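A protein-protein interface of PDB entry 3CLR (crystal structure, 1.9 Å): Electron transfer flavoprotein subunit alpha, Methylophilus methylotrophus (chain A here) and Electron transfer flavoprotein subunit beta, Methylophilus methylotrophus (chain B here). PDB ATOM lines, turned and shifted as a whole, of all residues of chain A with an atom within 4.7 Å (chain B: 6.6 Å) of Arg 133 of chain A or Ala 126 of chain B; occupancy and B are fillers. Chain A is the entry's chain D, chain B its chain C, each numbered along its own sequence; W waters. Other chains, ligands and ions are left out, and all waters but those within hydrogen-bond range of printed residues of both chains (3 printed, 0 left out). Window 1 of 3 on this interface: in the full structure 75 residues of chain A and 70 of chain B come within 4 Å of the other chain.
Hydrophobic or aromatic side chains of chain B that line the printed part of chain A: Tyr 127. Along chain B the printed residues that touch a printed residue of chain A span positions 124 to 129. Printed residues of chain A that touch a printed residue of chain B: Thr 117, Arg 133 and Gly 135. Among the printed residues, 7 pairs touch across the chains. Among the printed residues, no Asp or Glu carboxylate lies within 4 Å of a Lys or Arg side-chain nitrogen of the other chain.
O of Gln 125 of chain B is in hydrogen-bond range of NH1 of Arg 133 of chain A, at 2.8 Å. The backbone carbonyl oxygen of Ala 126 of chain B lies within hydrogen-bond range of the guanidinium group of Arg 133 of chain A (3.0 Å). O of Tyr 127 of chain B is in hydrogen-bond range of OG1 of Thr 117 of chain A (2.7 Å).
OD1 of Asp 124 of chain B lies within salt-bridge range of NZ of Lys 8 of chain B, at 2.8 Å. The backbone carbonyl oxygen of Tyr 127 of chain B is in hydrogen-bond range of the side-chain hydroxyl of Ser 129 of chain B. NE of Arg 133 of chain A sits at hydrogen-bond distance from O of Thr 117 of chain A (2.8 Å). The side-chain hydroxyl (OH) of Tyr 120 of chain A is in hydrogen-bond range of the backbone carbonyl oxygen (O) of Arg 133 of chain A (3.4 Å). O of Arg 133 of chain A lies within hydrogen-bond range of N of Val 142 of chain A, 2.7 Å away. The backbone carbonyl oxygen (O) of Val 140 of chain A is in hydrogen-bond range of the backbone NH (N) of Gly 135 of chain A.
Among the printed residues, merely in contact across the chains: Gly 135 of chain A with Gln 125 of chain B, Thr 117 of chain A with Ser 129 of chain B, Arg 133 of chain A with Tyr 127 of chain B and Gly 135 of chain A with Asp 124 of chain B.
Printed residues of chain B within 4 Å of Thr 117 of chain A: Tyr 127 (2.7 Å) and Ser 129 (3.4 Å). Thr 132 of chain A touches none of the printed residues of chain B. Printed residues of chain B within 4 Å of Gly 135 of chain A: Asp 124 and Gln 125. Of the printed residues of chain A, Asp 124 of chain B touches Gly 135 (3.7 Å). Printed residues of chain A within 4 Å of Gln 125 of chain B: Arg 133 (2.8 Å) and Gly 135 (3.1 Å). Of chain A, only Arg 133 comes within 4 Å of Ala 126 of chain B. Of the printed residues of chain A, Ser 129 of chain B touches Thr 117 (3.4 Å). The nearest residue of chain B that does not touch Arg 133 of chain A is Ala 128 of chain B (5.5 Å). The nearest residue of chain A that does not touch Ala 126 of chain B is Thr 117 of chain A (4.2 Å). The nearest printed residue of chain A that does not touch Gln 125 of chain B is Gly 134 of chain A (4.3 Å).
Water W1 lies within hydrogen-bond range of the side-chain carboxylate (OD2) of Asp 118 of chain A (2.7 Å), the backbone carbonyl oxygen (O) of Ala 126 of chain B (2.8 Å) and the guanidinium group (NH2) of Arg 133 of chain A (3.2 Å). Water W3 bridges O of Asp 124 of chain B (2.9 Å) and N of Gly 135 of chain A (3.4 Å). Water W2 lies within hydrogen-bond range of the backbone carbonyl oxygen (O) of Gln 125 of chain B (2.9 Å), the backbone carbonyl oxygen (O) of Gly 134 of chain A (3.0 Å) and the guanidinium group (NH1) of Arg 133 of chain A (3.4 Å).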
ATOM      1  N   THR A 117      -9.557   1.110  24.615  1.00  0.00           N
ATOM      2  CA  THR A 117     -10.407   1.624  23.543  1.00  0.00           C
ATOM      3  C   THR A 117     -11.058   0.563  22.655  1.00  0.00           C
ATOM      4  O   THR A 117     -10.587  -0.570  22.547  1.00  0.00           O
ATOM      5  CB  THR A 117      -9.660   2.622  22.613  1.00  0.00           C
ATOM      6  OG1 THR A 117      -8.620   1.961  21.895  1.00  0.00           O
ATOM      7  CG2 THR A 117      -9.107   3.793  23.394  1.00  0.00           C
ATOM      8  N   ASP A 118     -12.139   0.976  22.012  1.00  0.00           N
ATOM      9  CA  ASP A 118     -12.883   0.165  21.036  1.00  0.00           C
ATOM     10  C   ASP A 118     -13.205  -1.214  21.649  1.00  0.00           C
ATOM     11  O   ASP A 118     -13.010  -2.245  21.031  1.00  0.00           O
ATOM     12  CB  ASP A 118     -12.092   0.064  19.729  1.00  0.00           C
ATOM     13  CG  ASP A 118     -12.923  -0.478  18.561  1.00  0.00           C
ATOM     14  OD1 ASP A 118     -14.190  -0.387  18.580  1.00  0.00           O
ATOM     15  OD2 ASP A 118     -12.277  -0.991  17.627  1.00  0.00           O
ATOM     16  N   VAL A 119     -13.726  -1.169  22.874  1.00  0.00           N
ATOM     17  CA  VAL A 119     -14.022  -2.355  23.660  1.00  0.00           C
ATOM     18  C   VAL A 119     -15.366  -2.929  23.241  1.00  0.00           C
ATOM     19  O   VAL A 119     -16.329  -2.181  23.073  1.00  0.00           O
ATOM     20  CB  VAL A 119     -14.014  -2.016  25.173  1.00  0.00           C
ATOM     21  CG1 VAL A 119     -14.644  -3.145  26.002  1.00  0.00           C
ATOM     22  CG2 VAL A 119     -12.597  -1.757  25.631  1.00  0.00           C
ATOM     23  N   TYR A 120     -15.427  -4.253  23.073  1.00  0.00           N
ATOM     24  CA  TYR A 120     -16.674  -4.907  22.654  1.00  0.00           C
ATOM     25  C   TYR A 120     -17.141  -6.069  23.528  1.00  0.00           C
ATOM     26  O   TYR A 120     -18.190  -6.664  23.251  1.00  0.00           O
ATOM     27  CB  TYR A 120     -16.614  -5.309  21.171  1.00  0.00           C
ATOM     28  CG  TYR A 120     -15.428  -6.115  20.756  1.00  0.00           C
ATOM     29  CD1 TYR A 120     -15.362  -7.502  20.981  1.00  0.00           C
ATOM     30  CD2 TYR A 120     -14.355  -5.510  20.098  1.00  0.00           C
ATOM     31  CE1 TYR A 120     -14.248  -8.233  20.562  1.00  0.00           C
ATOM     32  CE2 TYR A 120     -13.249  -6.256  19.696  1.00  0.00           C
ATOM     33  CZ  TYR A 120     -13.213  -7.585  19.883  1.00  0.00           C
ATOM     34  OH  TYR A 120     -12.108  -8.305  19.438  1.00  0.00           O
ATOM     35  N   ALA A 131     -12.175  -6.109  30.308  1.00  0.00           N
ATOM     36  CA  ALA A 131     -12.596  -5.568  29.031  1.00  0.00           C
ATOM     37  C   ALA A 131     -11.901  -6.376  27.939  1.00  0.00           C
ATOM     38  O   ALA A 131     -10.760  -6.805  28.115  1.00  0.00           O
ATOM     39  CB  ALA A 131     -12.181  -4.122  28.928  1.00  0.00           C
ATOM     40  N   THR A 132     -12.592  -6.586  26.820  1.00  0.00           N
ATOM     41  CA  THR A 132     -11.979  -7.228  25.671  1.00  0.00           C
ATOM     42  C   THR A 132     -12.057  -6.332  24.441  1.00  0.00           C
ATOM     43  O   THR A 132     -13.079  -5.712  24.143  1.00  0.00           O
ATOM     44  CB  THR A 132     -12.635  -8.576  25.373  1.00  0.00           C
ATOM     45  OG1 THR A 132     -12.720  -9.333  26.596  1.00  0.00           O
ATOM     46  CG2 THR A 132     -11.852  -9.342  24.286  1.00  0.00           C
ATOM     47  N   ARG A 133     -10.948  -6.285  23.733  1.00  0.00           N
ATOM     48  CA  ARG A 133     -10.846  -5.554  22.460  1.00  0.00           C
ATOM     49  C   ARG A 133     -10.115  -6.463  21.463  1.00  0.00           C
ATOM     50  O   ARG A 133      -9.799  -7.611  21.772  1.00  0.00           O
ATOM     51  CB  ARG A 133     -10.099  -4.244  22.685  1.00  0.00           C
ATOM     52  CG  ARG A 133      -8.629  -4.435  23.019  1.00  0.00           C
ATOM     53  CD  ARG A 133      -7.908  -3.153  23.331  1.00  0.00           C
ATOM     54  NE  ARG A 133      -8.233  -2.051  22.444  1.00  0.00           N
ATOM     55  CZ  ARG A 133      -7.679  -1.862  21.242  1.00  0.00           C
ATOM     56  NH1 ARG A 133      -6.798  -2.743  20.754  1.00  0.00           N
ATOM     57  NH2 ARG A 133      -8.035  -0.816  20.499  1.00  0.00           N
ATOM     58  N   GLY A 134      -9.877  -5.957  20.251  1.00  0.00           N
ATOM     59  CA  GLY A 134      -9.245  -6.745  19.204  1.00  0.00           C
ATOM     60  C   GLY A 134      -7.751  -6.586  19.213  1.00  0.00           C
ATOM     61  O   GLY A 134      -7.227  -5.679  19.854  1.00  0.00           O
ATOM     62  N   GLY A 135      -7.072  -7.496  18.517  1.00  0.00           N
ATOM     63  CA  GLY A 135      -5.660  -7.321  18.166  1.00  0.00           C
ATOM     64  C   GLY A 135      -5.448  -7.804  16.741  1.00  0.00           C
ATOM     65  O   GLY A 135      -6.246  -8.621  16.199  1.00  0.00           O
ATOM     66  N   VAL A 140      -7.438 -11.522  16.645  1.00  0.00           N
ATOM     67  CA  VAL A 140      -7.491 -12.040  18.005  1.00  0.00           C
ATOM     68  C   VAL A 140      -8.362 -11.140  18.878  1.00  0.00           C
ATOM     69  O   VAL A 140      -8.650  -9.980  18.522  1.00  0.00           O
ATOM     70  CB  VAL A 140      -6.064 -12.177  18.640  1.00  0.00           C
ATOM     71  CG1 VAL A 140      -5.175 -13.184  17.866  1.00  0.00           C
ATOM     72  CG2 VAL A 140      -5.385 -10.813  18.773  1.00  0.00           C
ATOM     73  N   ASN A 141      -8.781 -11.688  20.017  1.00  0.00           N
ATOM     74  CA  ASN A 141      -9.267 -10.929  21.136  1.00  0.00           C
ATOM     75  C   ASN A 141      -8.123 -10.726  22.147  1.00  0.00           C
ATOM     76  O   ASN A 141      -7.337 -11.642  22.436  1.00  0.00           O
ATOM     77  CB  ASN A 141     -10.427 -11.646  21.844  1.00  0.00           C
ATOM     78  CG  ASN A 141     -11.768 -11.483  21.128  1.00  0.00           C
ATOM     79  OD1 ASN A 141     -12.807 -11.983  21.616  1.00  0.00           O
ATOM     80  ND2 ASN A 141     -11.757 -10.857  19.971  1.00  0.00           N
ATOM     81  N   VAL A 142      -8.059  -9.516  22.688  1.00  0.00           N
ATOM     82  CA  VAL A 142      -7.114  -9.185  23.734  1.00  0.00           C
ATOM     83  C   VAL A 142      -7.932  -8.793  24.950  1.00  0.00           C
ATOM     84  O   VAL A 142      -8.676  -7.815  24.913  1.00  0.00           O
ATOM     85  CB  VAL A 142      -6.198  -8.000  23.368  1.00  0.00           C
ATOM     86  CG1 VAL A 142      -5.147  -7.778  24.446  1.00  0.00           C
ATOM     87  CG2 VAL A 142      -5.534  -8.222  21.984  1.00  0.00           C
ATOM     88  N   LYS B   8       4.685   4.191  12.976  1.00  0.00           N
ATOM     89  CA  LYS B   8       4.712   2.845  13.536  1.00  0.00           C
ATOM     90  C   LYS B   8       4.864   1.796  12.414  1.00  0.00           C
ATOM     91  O   LYS B   8       4.209   1.840  11.367  1.00  0.00           O
ATOM     92  CB  LYS B   8       3.423   2.542  14.312  1.00  0.00           C
ATOM     93  CG  LYS B   8       3.477   1.241  15.055  1.00  0.00           C
ATOM     94  CD  LYS B   8       2.165   0.878  15.729  1.00  0.00           C
ATOM     95  CE  LYS B   8       2.282  -0.463  16.412  1.00  0.00           C
ATOM     96  NZ  LYS B   8       0.971  -0.886  17.115  1.00  0.00           N
ATOM     97  N   GLN B 121      -4.940   5.829  13.537  1.00  0.00           N
ATOM     98  CA  GLN B 121      -4.817   4.577  14.271  1.00  0.00           C
ATOM     99  C   GLN B 121      -3.807   3.659  13.583  1.00  0.00           C
ATOM    100  O   GLN B 121      -3.320   3.963  12.474  1.00  0.00           O
ATOM    101  CB  GLN B 121      -6.171   3.883  14.411  1.00  0.00           C
ATOM    102  CG  GLN B 121      -6.723   3.337  13.104  1.00  0.00           C
ATOM    103  CD  GLN B 121      -8.055   2.635  13.275  1.00  0.00           C
ATOM    104  OE1 GLN B 121      -8.268   1.562  12.710  1.00  0.00           O
ATOM    105  NE2 GLN B 121      -8.921   3.200  14.092  1.00  0.00           N
ATOM    106  N   SER B 122      -3.424   2.578  14.292  1.00  0.00           N
ATOM    107  CA  SER B 122      -2.560   1.523  13.744  1.00  0.00           C
ATOM    108  C   SER B 122      -3.415   0.392  13.190  1.00  0.00           C
ATOM    109  O   SER B 122      -4.460   0.069  13.760  1.00  0.00           O
ATOM    110  CB  SER B 122      -1.591   0.947  14.787  1.00  0.00           C
ATOM    111  OG  SER B 122      -2.234   0.629  15.999  1.00  0.00           O
ATOM    112  N   SER B 123      -2.982  -0.177  12.069  1.00  0.00           N
ATOM    113  CA  SER B 123      -3.722  -1.270  11.443  1.00  0.00           C
ATOM    114  C   SER B 123      -3.717  -2.536  12.282  1.00  0.00           C
ATOM    115  O   SER B 123      -4.641  -3.346  12.143  1.00  0.00           O
ATOM    116  CB  SER B 123      -3.175  -1.606  10.063  1.00  0.00           C
ATOM    117  OG  SER B 123      -1.803  -1.954  10.179  1.00  0.00           O
ATOM    118  N   ASP B 124      -2.706  -2.717  13.141  1.00  0.00           N
ATOM    119  CA  ASP B 124      -2.672  -3.882  13.992  1.00  0.00           C
ATOM    120  C   ASP B 124      -3.556  -3.759  15.240  1.00  0.00           C
ATOM    121  O   ASP B 124      -4.578  -4.447  15.354  1.00  0.00           O
ATOM    122  CB  ASP B 124      -1.239  -4.360  14.330  1.00  0.00           C
ATOM    123  CG  ASP B 124      -0.276  -3.250  14.778  1.00  0.00           C
ATOM    124  OD1 ASP B 124      -0.697  -2.141  15.205  1.00  0.00           O
ATOM    125  OD2 ASP B 124       0.944  -3.546  14.744  1.00  0.00           O
ATOM    126  N   GLN B 125      -3.203  -2.864  16.148  1.00  0.00           N
ATOM    127  CA  GLN B 125      -3.962  -2.732  17.387  1.00  0.00           C
ATOM    128  C   GLN B 125      -5.135  -1.731  17.339  1.00  0.00           C
ATOM    129  O   GLN B 125      -6.088  -1.857  18.146  1.00  0.00           O
ATOM    130  CB  GLN B 125      -3.015  -2.460  18.557  1.00  0.00           C
ATOM    131  CG  GLN B 125      -1.881  -3.566  18.775  1.00  0.00           C
ATOM    132  CD  GLN B 125      -2.079  -5.015  18.145  1.00  0.00           C
ATOM    133  OE1 GLN B 125      -3.144  -5.590  18.118  1.00  0.00           O
ATOM    134  NE2 GLN B 125      -0.983  -5.596  17.720  1.00  0.00           N
ATOM    135  N   ALA B 126      -5.091  -0.758  16.418  1.00  0.00           N
ATOM    136  CA  ALA B 126      -6.172   0.180  16.257  1.00  0.00           C
ATOM    137  C   ALA B 126      -6.628   0.734  17.601  1.00  0.00           C
ATOM    138  O   ALA B 126      -7.821   0.689  17.937  1.00  0.00           O
ATOM    139  CB  ALA B 126      -7.316  -0.471  15.526  1.00  0.00           C
ATOM    140  N   TYR B 127      -5.665   1.250  18.366  1.00  0.00           N
ATOM    141  CA  TYR B 127      -5.966   1.894  19.623  1.00  0.00           C
ATOM    142  C   TYR B 127      -6.621   3.252  19.369  1.00  0.00           C
ATOM    143  O   TYR B 127      -7.414   3.691  20.200  1.00  0.00           O
ATOM    144  CB  TYR B 127      -4.721   2.179  20.452  1.00  0.00           C
ATOM    145  CG  TYR B 127      -3.933   0.971  20.866  1.00  0.00           C
ATOM    146  CD1 TYR B 127      -2.581   0.871  20.582  1.00  0.00           C
ATOM    147  CD2 TYR B 127      -4.534  -0.064  21.587  1.00  0.00           C
ATOM    148  CE1 TYR B 127      -1.819  -0.235  20.996  1.00  0.00           C
ATOM    149  CE2 TYR B 127      -3.799  -1.192  21.986  1.00  0.00           C
ATOM    150  CZ  TYR B 127      -2.441  -1.287  21.681  1.00  0.00           C
ATOM    151  OH  TYR B 127      -1.691  -2.429  22.066  1.00  0.00           O
ATOM    152  N   ALA B 128      -6.238   3.892  18.256  1.00  0.00           N
ATOM    153  CA  ALA B 128      -6.582   5.293  17.941  1.00  0.00           C
ATOM    154  C   ALA B 128      -6.375   6.196  19.184  1.00  0.00           C
ATOM    155  O   ALA B 128      -7.303   6.922  19.599  1.00  0.00           O
ATOM    156  CB  ALA B 128      -7.986   5.389  17.440  1.00  0.00           C
ATOM    157  N   SER B 129      -5.170   6.093  19.764  1.00  0.00           N
ATOM    158  CA  SER B 129      -4.837   6.733  21.032  1.00  0.00           C
ATOM    159  C   SER B 129      -3.505   7.435  21.109  1.00  0.00           C
ATOM    160  O   SER B 129      -3.345   8.368  21.884  1.00  0.00           O
ATOM    161  CB  SER B 129      -4.816   5.687  22.152  1.00  0.00           C
ATOM    162  OG  SER B 129      -6.108   5.219  22.464  1.00  0.00           O
ATOM    163  N   SER B 227      -3.486  -0.427  31.072  1.00  0.00           N
ATOM    164  CA  SER B 227      -4.274  -1.656  31.199  1.00  0.00           C
ATOM    165  C   SER B 227      -3.265  -2.786  31.130  1.00  0.00           C
ATOM    166  O   SER B 227      -2.158  -2.590  30.619  1.00  0.00           O
ATOM    167  CB  SER B 227      -5.327  -1.777  30.099  1.00  0.00           C
ATOM    168  OG  SER B 227      -4.764  -2.003  28.808  1.00  0.00           O
HETATM  169  O   HOH W   1      -9.646  -1.479  17.772  1.00  0.00           O
HETATM  170  O   HOH W   2      -8.329  -3.734  17.911  1.00  0.00           O
HETATM  171  O   HOH W   3      -7.248  -5.265  15.981  1.00  0.00           O
